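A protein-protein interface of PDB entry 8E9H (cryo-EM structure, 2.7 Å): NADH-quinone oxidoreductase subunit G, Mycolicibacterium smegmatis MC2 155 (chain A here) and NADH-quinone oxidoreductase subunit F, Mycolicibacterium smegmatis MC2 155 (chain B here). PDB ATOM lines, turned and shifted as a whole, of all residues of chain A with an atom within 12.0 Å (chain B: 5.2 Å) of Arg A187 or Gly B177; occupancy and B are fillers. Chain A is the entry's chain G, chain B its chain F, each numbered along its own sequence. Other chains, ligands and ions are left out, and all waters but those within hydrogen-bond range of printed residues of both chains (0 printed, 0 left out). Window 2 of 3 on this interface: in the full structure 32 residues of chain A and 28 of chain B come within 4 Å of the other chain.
C of Met A185 touches NH1 of Arg B195, 3.7 Å away.
CA of Ala B178 touches NH1 of Arg A187, at 3.5 Å.
Ser B350 touches Arg A187.
Cys B351 touches Arg A187.
N of Gly A188 touches N of Gly B352 (3.8 Å).
NH1 of Arg A187 lies within hydrogen-bond range of O of Gly B177 (3.0 Å).
The backbone NH (N) of Gly A188 lies within hydrogen-bond range of the backbone carbonyl oxygen (O) of Ser B350 (2.9 Å).
The side-chain amide nitrogen (NE2) of Gln A191 is in hydrogen-bond range of the backbone carbonyl oxygen (O) of Gly B352 (3.0 Å).
NH2 of Arg B195 lies within hydrogen-bond range of OE1 of Gln A191 (2.4 Å).
The guanidinium group (NH2) of Arg A187 is in hydrogen-bond range of the backbone carbonyl oxygen (O) of His B348, at 2.9 Å.
O of Cys B351 sits close to OE1 of Gln A191 (3.2 Å).
NH2 of Arg B195 is in hydrogen-bond range of O of Glu A186 (2.6 Å).
NH1 of Arg B195 lies within hydrogen-bond range of O of Leu A184 (2.7 Å).
The backbone NH (N) of Gly A188 is in hydrogen-bond range of the backbone carbonyl oxygen (O) of Cys B351 (3.2 Å).
The backbone NH (N) of Met A185 is in hydrogen-bond range of the backbone carbonyl oxygen (O) of Gln A192 (2.8 Å).
Asp A183 touches none of the printed residues of chain B.
Of the printed residues of chain B, Leu A184 touches Arg B195.
Of the printed residues of chain B, Met A185 touches Arg B195.
Printed residues of chain B within 4 Å of Gly A188: Ser B350 (2.9 Å), Cys B351 (3.2 Å) and Gly B352 (3.8 Å).
Of the printed residues of chain A, Gly B177 touches Arg A187.
Ala B178 touches just one residue of chain A: Arg A187.
His B348 touches just one residue of chain A: Arg A187 (2.9 Å).
No residue of chain A comes within 4 Å of Glu B349.
Of chain A, only Arg A187 (3.1 Å) and Gly A188 (2.9 Å) come within 4 Å of Ser B350.
Cys B351 touches just these residues of chain A: Arg A187 (3.7 Å), Gly A188 (3.2 Å) and Gln A191 (3.2 Å).
Gly B352 touches two residues of chain A.
Of the 19 printed residues of chain A, 6 touch a printed residue of chain B.
Hydrophobic or aromatic side chains of chain B that line the printed part of chain A: Ala B178 and His B348.
Along chain B the printed residues that touch a printed residue of chain A span positions 177 to 352.
Among the printed residues, no Asp or Glu carboxylate lies within 4 Å of a Lys or Arg side-chain nitrogen of the other chain.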
ATOM      1  N   ASN A 109       3.647  16.624  10.845  1.00  0.00           N
ATOM      2  CA  ASN A 109       3.360  15.557  11.791  1.00  0.00           C
ATOM      3  C   ASN A 109       2.525  14.441  11.190  1.00  0.00           C
ATOM      4  O   ASN A 109       2.305  13.426  11.856  1.00  0.00           O
ATOM      5  CB  ASN A 109       2.637  16.127  13.011  1.00  0.00           C
ATOM      6  CG  ASN A 109       3.587  16.545  14.105  1.00  0.00           C
ATOM      7  OD1 ASN A 109       4.641  15.943  14.291  1.00  0.00           O
ATOM      8  ND2 ASN A 109       3.219  17.586  14.838  1.00  0.00           N
ATOM      9  N   ARG A 144       5.329  13.562  15.509  1.00  0.00           N
ATOM     10  CA  ARG A 144       4.465  13.151  16.604  1.00  0.00           C
ATOM     11  C   ARG A 144       3.861  11.791  16.294  1.00  0.00           C
ATOM     12  O   ARG A 144       3.573  11.474  15.139  1.00  0.00           O
ATOM     13  CB  ARG A 144       3.358  14.182  16.806  1.00  0.00           C
ATOM     14  CG  ARG A 144       2.334  13.813  17.855  1.00  0.00           C
ATOM     15  CD  ARG A 144       1.222  14.834  17.884  1.00  0.00           C
ATOM     16  NE  ARG A 144       0.422  14.770  16.668  1.00  0.00           N
ATOM     17  CZ  ARG A 144      -0.083  15.818  16.031  1.00  0.00           C
ATOM     18  NH1 ARG A 144       0.125  17.054  16.453  1.00  0.00           N
ATOM     19  NH2 ARG A 144      -0.814  15.621  14.938  1.00  0.00           N
ATOM     20  N   THR A 145       3.662  10.983  17.329  1.00  0.00           N
ATOM     21  CA  THR A 145       3.137   9.643  17.139  1.00  0.00           C
ATOM     22  C   THR A 145       2.166   9.294  18.257  1.00  0.00           C
ATOM     23  O   THR A 145       2.334   9.712  19.404  1.00  0.00           O
ATOM     24  CB  THR A 145       4.267   8.608  17.083  1.00  0.00           C
ATOM     25  OG1 THR A 145       3.710   7.293  16.994  1.00  0.00           O
ATOM     26  CG2 THR A 145       5.141   8.702  18.317  1.00  0.00           C
ATOM     27  N   PHE A 146       1.148   8.520  17.898  1.00  0.00           N
ATOM     28  CA  PHE A 146       0.140   8.009  18.808  1.00  0.00           C
ATOM     29  C   PHE A 146      -0.055   6.532  18.519  1.00  0.00           C
ATOM     30  O   PHE A 146       0.186   6.087  17.390  1.00  0.00           O
ATOM     31  CB  PHE A 146      -1.212   8.718  18.640  1.00  0.00           C
ATOM     32  CG  PHE A 146      -1.201  10.159  19.030  1.00  0.00           C
ATOM     33  CD1 PHE A 146      -1.301  10.532  20.353  1.00  0.00           C
ATOM     34  CD2 PHE A 146      -1.111  11.144  18.069  1.00  0.00           C
ATOM     35  CE1 PHE A 146      -1.301  11.858  20.711  1.00  0.00           C
ATOM     36  CE2 PHE A 146      -1.110  12.471  18.420  1.00  0.00           C
ATOM     37  CZ  PHE A 146      -1.205  12.829  19.742  1.00  0.00           C
ATOM     38  N   ARG A 160      -5.226   8.837  15.519  1.00  0.00           N
ATOM     39  CA  ARG A 160      -4.997  10.218  15.922  1.00  0.00           C
ATOM     40  C   ARG A 160      -3.824  10.855  15.198  1.00  0.00           C
ATOM     41  O   ARG A 160      -3.795  12.079  15.056  1.00  0.00           O
ATOM     42  CB  ARG A 160      -4.770  10.289  17.425  1.00  0.00           C
ATOM     43  CG  ARG A 160      -6.021  10.048  18.225  1.00  0.00           C
ATOM     44  CD  ARG A 160      -5.694   9.692  19.645  1.00  0.00           C
ATOM     45  NE  ARG A 160      -5.037   8.397  19.733  1.00  0.00           N
ATOM     46  CZ  ARG A 160      -4.546   7.892  20.853  1.00  0.00           C
ATOM     47  NH1 ARG A 160      -4.631   8.546  21.996  1.00  0.00           N
ATOM     48  NH2 ARG A 160      -3.960   6.699  20.824  1.00  0.00           N
ATOM     49  N   CYS A 163      -5.008  12.759  12.367  1.00  0.00           N
ATOM     50  CA  CYS A 163      -5.938  13.829  12.693  1.00  0.00           C
ATOM     51  C   CYS A 163      -5.303  15.186  12.444  1.00  0.00           C
ATOM     52  O   CYS A 163      -4.181  15.450  12.881  1.00  0.00           O
ATOM     53  CB  CYS A 163      -6.374  13.719  14.151  1.00  0.00           C
ATOM     54  SG  CYS A 163      -7.477  15.026  14.680  1.00  0.00           S
ATOM     55  N   LEU A 165      -7.014  17.783  13.559  1.00  0.00           N
ATOM     56  CA  LEU A 165      -7.648  18.559  14.618  1.00  0.00           C
ATOM     57  C   LEU A 165      -8.525  19.662  14.041  1.00  0.00           C
ATOM     58  O   LEU A 165      -8.544  20.790  14.532  1.00  0.00           O
ATOM     59  CB  LEU A 165      -6.603  19.136  15.568  1.00  0.00           C
ATOM     60  CG  LEU A 165      -5.913  18.072  16.415  1.00  0.00           C
ATOM     61  CD1 LEU A 165      -4.568  18.557  16.899  1.00  0.00           C
ATOM     62  CD2 LEU A 165      -6.792  17.692  17.582  1.00  0.00           C
ATOM     63  N   ASP A 183     -14.604  14.410  22.090  1.00  0.00           N
ATOM     64  CA  ASP A 183     -14.211  15.805  22.204  1.00  0.00           C
ATOM     65  C   ASP A 183     -12.698  15.895  22.111  1.00  0.00           C
ATOM     66  O   ASP A 183     -11.989  14.892  22.191  1.00  0.00           O
ATOM     67  CB  ASP A 183     -14.728  16.420  23.501  1.00  0.00           C
ATOM     68  CG  ASP A 183     -14.750  17.930  23.456  1.00  0.00           C
ATOM     69  OD1 ASP A 183     -14.094  18.503  22.562  1.00  0.00           O
ATOM     70  OD2 ASP A 183     -15.427  18.545  24.303  1.00  0.00           O
ATOM     71  N   LEU A 184     -12.214  17.118  21.926  1.00  0.00           N
ATOM     72  CA  LEU A 184     -10.786  17.357  21.785  1.00  0.00           C
ATOM     73  C   LEU A 184     -10.124  17.313  23.155  1.00  0.00           C
ATOM     74  O   LEU A 184     -10.283  18.234  23.961  1.00  0.00           O
ATOM     75  CB  LEU A 184     -10.544  18.697  21.105  1.00  0.00           C
ATOM     76  CG  LEU A 184     -11.104  18.818  19.688  1.00  0.00           C
ATOM     77  CD1 LEU A 184     -10.698  20.142  19.087  1.00  0.00           C
ATOM     78  CD2 LEU A 184     -10.631  17.678  18.813  1.00  0.00           C
ATOM     79  N   MET A 185      -9.388  16.243  23.411  1.00  0.00           N
ATOM     80  CA  MET A 185      -8.730  15.980  24.672  1.00  0.00           C
ATOM     81  C   MET A 185      -7.330  16.582  24.638  1.00  0.00           C
ATOM     82  O   MET A 185      -6.795  16.913  23.577  1.00  0.00           O
ATOM     83  CB  MET A 185      -8.640  14.474  24.891  1.00  0.00           C
ATOM     84  CG  MET A 185      -9.981  13.792  25.020  1.00  0.00           C
ATOM     85  SD  MET A 185     -11.010  14.244  26.409  1.00  0.00           S
ATOM     86  CE  MET A 185     -12.493  13.363  25.936  1.00  0.00           C
ATOM     87  N   GLU A 186      -6.719  16.695  25.815  1.00  0.00           N
ATOM     88  CA  GLU A 186      -5.335  17.140  25.922  1.00  0.00           C
ATOM     89  C   GLU A 186      -5.169  18.563  25.411  1.00  0.00           C
ATOM     90  O   GLU A 186      -6.156  19.248  25.132  1.00  0.00           O
ATOM     91  CB  GLU A 186      -4.409  16.196  25.154  1.00  0.00           C
ATOM     92  CG  GLU A 186      -4.496  14.751  25.588  1.00  0.00           C
ATOM     93  CD  GLU A 186      -3.921  14.524  26.966  1.00  0.00           C
ATOM     94  OE1 GLU A 186      -3.280  15.452  27.502  1.00  0.00           O
ATOM     95  OE2 GLU A 186      -4.101  13.417  27.513  1.00  0.00           O
ATOM     96  N   ARG A 187      -3.923  19.013  25.286  1.00  0.00           N
ATOM     97  CA  ARG A 187      -3.622  20.383  24.908  1.00  0.00           C
ATOM     98  C   ARG A 187      -2.391  20.414  24.016  1.00  0.00           C
ATOM     99  O   ARG A 187      -1.554  19.511  24.054  1.00  0.00           O
ATOM    100  CB  ARG A 187      -3.384  21.255  26.141  1.00  0.00           C
ATOM    101  CG  ARG A 187      -3.245  22.719  25.831  1.00  0.00           C
ATOM    102  CD  ARG A 187      -3.101  23.539  27.087  1.00  0.00           C
ATOM    103  NE  ARG A 187      -1.800  23.343  27.711  1.00  0.00           N
ATOM    104  CZ  ARG A 187      -1.519  23.653  28.967  1.00  0.00           C
ATOM    105  NH1 ARG A 187      -2.430  24.175  29.771  1.00  0.00           N
ATOM    106  NH2 ARG A 187      -0.293  23.436  29.429  1.00  0.00           N
ATOM    107  N   GLY A 188      -2.292  21.468  23.211  1.00  0.00           N
ATOM    108  CA  GLY A 188      -1.106  21.658  22.396  1.00  0.00           C
ATOM    109  C   GLY A 188      -0.944  20.553  21.374  1.00  0.00           C
ATOM    110  O   GLY A 188      -1.917  19.982  20.875  1.00  0.00           O
ATOM    111  N   ALA A 189       0.313  20.237  21.061  1.00  0.00           N
ATOM    112  CA  ALA A 189       0.586  19.205  20.069  1.00  0.00           C
ATOM    113  C   ALA A 189      -0.004  17.867  20.482  1.00  0.00           C
ATOM    114  O   ALA A 189      -0.222  16.997  19.635  1.00  0.00           O
ATOM    115  CB  ALA A 189       2.091  19.070  19.853  1.00  0.00           C
ATOM    116  N   LEU A 190      -0.265  17.684  21.773  1.00  0.00           N
ATOM    117  CA  LEU A 190      -0.855  16.450  22.261  1.00  0.00           C
ATOM    118  C   LEU A 190      -2.370  16.430  22.131  1.00  0.00           C
ATOM    119  O   LEU A 190      -2.985  15.407  22.444  1.00  0.00           O
ATOM    120  CB  LEU A 190      -0.461  16.237  23.722  1.00  0.00           C
ATOM    121  CG  LEU A 190      -0.670  14.836  24.294  1.00  0.00           C
ATOM    122  CD1 LEU A 190       0.191  13.825  23.567  1.00  0.00           C
ATOM    123  CD2 LEU A 190      -0.367  14.828  25.781  1.00  0.00           C
ATOM    124  N   GLN A 191      -2.986  17.520  21.677  1.00  0.00           N
ATOM    125  CA  GLN A 191      -4.434  17.551  21.544  1.00  0.00           C
ATOM    126  C   GLN A 191      -4.896  16.458  20.594  1.00  0.00           C
ATOM    127  O   GLN A 191      -4.262  16.198  19.570  1.00  0.00           O
ATOM    128  CB  GLN A 191      -4.898  18.914  21.040  1.00  0.00           C
ATOM    129  CG  GLN A 191      -6.398  19.074  21.075  1.00  0.00           C
ATOM    130  CD  GLN A 191      -6.843  20.465  20.707  1.00  0.00           C
ATOM    131  OE1 GLN A 191      -7.392  21.189  21.532  1.00  0.00           O
ATOM    132  NE2 GLN A 191      -6.613  20.847  19.461  1.00  0.00           N
ATOM    133  N   GLN A 192      -6.003  15.809  20.939  1.00  0.00           N
ATOM    134  CA  GLN A 192      -6.433  14.646  20.180  1.00  0.00           C
ATOM    135  C   GLN A 192      -7.908  14.391  20.425  1.00  0.00           C
ATOM    136  O   GLN A 192      -8.366  14.417  21.561  1.00  0.00           O
ATOM    137  CB  GLN A 192      -5.632  13.411  20.582  1.00  0.00           C
ATOM    138  CG  GLN A 192      -5.831  13.037  22.034  1.00  0.00           C
ATOM    139  CD  GLN A 192      -4.783  12.085  22.539  1.00  0.00           C
ATOM    140  OE1 GLN A 192      -5.010  10.879  22.611  1.00  0.00           O
ATOM    141  NE2 GLN A 192      -3.623  12.615  22.892  1.00  0.00           N
ATOM    142  N   VAL A 193      -8.652  14.128  19.356  1.00  0.00           N
ATOM    143  CA  VAL A 193     -10.039  13.730  19.538  1.00  0.00           C
ATOM    144  C   VAL A 193     -10.082  12.434  20.333  1.00  0.00           C
ATOM    145  O   VAL A 193      -9.244  11.542  20.154  1.00  0.00           O
ATOM    146  CB  VAL A 193     -10.751  13.576  18.184  1.00  0.00           C
ATOM    147  CG1 VAL A 193     -10.117  12.472  17.381  1.00  0.00           C
ATOM    148  CG2 VAL A 193     -12.220  13.286  18.399  1.00  0.00           C
ATOM    149  N   GLY A 194     -11.051  12.325  21.235  1.00  0.00           N
ATOM    150  CA  GLY A 194     -11.152  11.126  22.043  1.00  0.00           C
ATOM    151  C   GLY A 194     -12.459  11.036  22.790  1.00  0.00           C
ATOM    152  O   GLY A 194     -13.154  12.033  23.006  1.00  0.00           O
ATOM    153  N   GLU B 136      -1.762  28.459  40.129  1.00  0.00           N
ATOM    154  CA  GLU B 136      -0.399  28.233  40.591  1.00  0.00           C
ATOM    155  C   GLU B 136       0.105  29.317  41.532  1.00  0.00           C
ATOM    156  O   GLU B 136       1.297  29.320  41.852  1.00  0.00           O
ATOM    157  CB  GLU B 136       0.545  28.126  39.395  1.00  0.00           C
ATOM    158  CG  GLU B 136       0.118  27.108  38.362  1.00  0.00           C
ATOM    159  CD  GLU B 136      -0.454  27.749  37.121  1.00  0.00           C
ATOM    160  OE1 GLU B 136      -1.300  28.657  37.256  1.00  0.00           O
ATOM    161  OE2 GLU B 136      -0.057  27.349  36.007  1.00  0.00           O
ATOM    162  N   GLY B 175      -8.654  29.456  38.460  1.00  0.00           N
ATOM    163  CA  GLY B 175      -8.424  28.704  37.247  1.00  0.00           C
ATOM    164  C   GLY B 175      -7.271  27.732  37.390  1.00  0.00           C
ATOM    165  O   GLY B 175      -6.354  27.915  38.188  1.00  0.00           O
ATOM    166  N   ALA B 176      -7.328  26.676  36.590  1.00  0.00           N
ATOM    167  CA  ALA B 176      -6.266  25.689  36.560  1.00  0.00           C
ATOM    168  C   ALA B 176      -5.149  26.155  35.633  1.00  0.00           C
ATOM    169  O   ALA B 176      -5.204  27.233  35.040  1.00  0.00           O
ATOM    170  CB  ALA B 176      -6.806  24.333  36.123  1.00  0.00           C
ATOM    171  N   GLY B 177      -4.121  25.324  35.515  1.00  0.00           N
ATOM    172  CA  GLY B 177      -2.912  25.725  34.826  1.00  0.00           C
ATOM    173  C   GLY B 177      -3.061  25.815  33.325  1.00  0.00           C
ATOM    174  O   GLY B 177      -3.135  24.792  32.639  1.00  0.00           O
ATOM    175  N   ALA B 178      -3.096  27.035  32.801  1.00  0.00           N
ATOM    176  CA  ALA B 178      -3.143  27.243  31.359  1.00  0.00           C
ATOM    177  C   ALA B 178      -2.799  28.692  31.074  1.00  0.00           C
ATOM    178  O   ALA B 178      -3.548  29.591  31.463  1.00  0.00           O
ATOM    179  CB  ALA B 178      -4.518  26.893  30.803  1.00  0.00           C
ATOM    180  N   TYR B 179      -1.678  28.920  30.392  1.00  0.00           N
ATOM    181  CA  TYR B 179      -1.306  30.282  30.036  1.00  0.00           C
ATOM    182  C   TYR B 179      -2.332  30.899  29.100  1.00  0.00           C
ATOM    183  O   TYR B 179      -2.713  32.064  29.262  1.00  0.00           O
ATOM    184  CB  TYR B 179       0.078  30.288  29.392  1.00  0.00           C
ATOM    185  CG  TYR B 179       0.406  31.551  28.637  1.00  0.00           C
ATOM    186  CD1 TYR B 179       0.257  32.794  29.227  1.00  0.00           C
ATOM    187  CD2 TYR B 179       0.881  31.499  27.338  1.00  0.00           C
ATOM    188  CE1 TYR B 179       0.563  33.947  28.541  1.00  0.00           C
ATOM    189  CE2 TYR B 179       1.189  32.646  26.647  1.00  0.00           C
ATOM    190  CZ  TYR B 179       1.030  33.866  27.253  1.00  0.00           C
ATOM    191  OH  TYR B 179       1.336  35.014  26.565  1.00  0.00           O
ATOM    192  N   ILE B 180      -2.805  30.127  28.120  1.00  0.00           N
ATOM    193  CA  ILE B 180      -3.718  30.668  27.121  1.00  0.00           C
ATOM    194  C   ILE B 180      -4.980  31.206  27.771  1.00  0.00           C
ATOM    195  O   ILE B 180      -5.619  32.122  27.240  1.00  0.00           O
ATOM    196  CB  ILE B 180      -4.047  29.596  26.065  1.00  0.00           C
ATOM    197  CG1 ILE B 180      -5.001  30.155  25.012  1.00  0.00           C
ATOM    198  CG2 ILE B 180      -4.670  28.381  26.719  1.00  0.00           C
ATOM    199  CD1 ILE B 180      -4.503  31.405  24.339  1.00  0.00           C
ATOM    200  N   ARG B 195     -12.843  24.080  27.620  1.00  0.00           N
ATOM    201  CA  ARG B 195     -11.430  24.196  27.307  1.00  0.00           C
ATOM    202  C   ARG B 195     -11.067  25.660  27.117  1.00  0.00           C
ATOM    203  O   ARG B 195     -11.776  26.412  26.448  1.00  0.00           O
ATOM    204  CB  ARG B 195     -11.099  23.404  26.046  1.00  0.00           C
ATOM    205  CG  ARG B 195     -11.318  21.917  26.174  1.00  0.00           C
ATOM    206  CD  ARG B 195     -11.254  21.248  24.820  1.00  0.00           C
ATOM    207  NE  ARG B 195      -9.945  21.401  24.201  1.00  0.00           N
ATOM    208  CZ  ARG B 195      -8.862  20.730  24.565  1.00  0.00           C
ATOM    209  NH1 ARG B 195      -8.894  19.849  25.551  1.00  0.00           N
ATOM    210  NH2 ARG B 195      -7.718  20.948  23.926  1.00  0.00           N
ATOM    211  N   HIS B 348       4.293  24.033  25.053  1.00  0.00           N
ATOM    212  CA  HIS B 348       3.585  23.485  26.201  1.00  0.00           C
ATOM    213  C   HIS B 348       2.295  24.241  26.483  1.00  0.00           C
ATOM    214  O   HIS B 348       1.379  23.689  27.102  1.00  0.00           O
ATOM    215  CB  HIS B 348       4.495  23.521  27.425  1.00  0.00           C
ATOM    216  CG  HIS B 348       3.867  22.961  28.660  1.00  0.00           C
ATOM    217  ND1 HIS B 348       3.692  21.609  28.858  1.00  0.00           N
ATOM    218  CD2 HIS B 348       3.372  23.570  29.762  1.00  0.00           C
ATOM    219  CE1 HIS B 348       3.118  21.409  30.029  1.00  0.00           C
ATOM    220  NE2 HIS B 348       2.912  22.583  30.599  1.00  0.00           N
ATOM    221  N   GLU B 349       2.202  25.495  26.047  1.00  0.00           N
ATOM    222  CA  GLU B 349       1.085  26.357  26.399  1.00  0.00           C
ATOM    223  C   GLU B 349       0.081  26.548  25.271  1.00  0.00           C
ATOM    224  O   GLU B 349      -1.016  27.051  25.527  1.00  0.00           O
ATOM    225  CB  GLU B 349       1.605  27.726  26.846  1.00  0.00           C
ATOM    226  N   SER B 350       0.421  26.177  24.040  1.00  0.00           N
ATOM    227  CA  SER B 350      -0.531  26.279  22.943  1.00  0.00           C
ATOM    228  C   SER B 350      -1.749  25.422  23.229  1.00  0.00           C
ATOM    229  O   SER B 350      -1.622  24.266  23.635  1.00  0.00           O
ATOM    230  CB  SER B 350       0.120  25.831  21.637  1.00  0.00           C
ATOM    231  OG  SER B 350       1.062  26.785  21.191  1.00  0.00           O
ATOM    232  N   CYS B 351      -2.940  25.983  23.015  1.00  0.00           N
ATOM    233  CA  CYS B 351      -4.134  25.193  23.287  1.00  0.00           C
ATOM    234  C   CYS B 351      -4.317  24.104  22.242  1.00  0.00           C
ATOM    235  O   CYS B 351      -5.002  23.112  22.500  1.00  0.00           O
ATOM    236  CB  CYS B 351      -5.377  26.073  23.344  1.00  0.00           C
ATOM    237  SG  CYS B 351      -5.839  26.852  21.813  1.00  0.00           S
ATOM    238  N   GLY B 352      -3.713  24.264  21.069  1.00  0.00           N
ATOM    239  CA  GLY B 352      -3.781  23.273  20.017  1.00  0.00           C
ATOM    240  C   GLY B 352      -4.834  23.540  18.969  1.00  0.00           C
ATOM    241  O   GLY B 352      -4.873  22.824  17.964  1.00  0.00           O
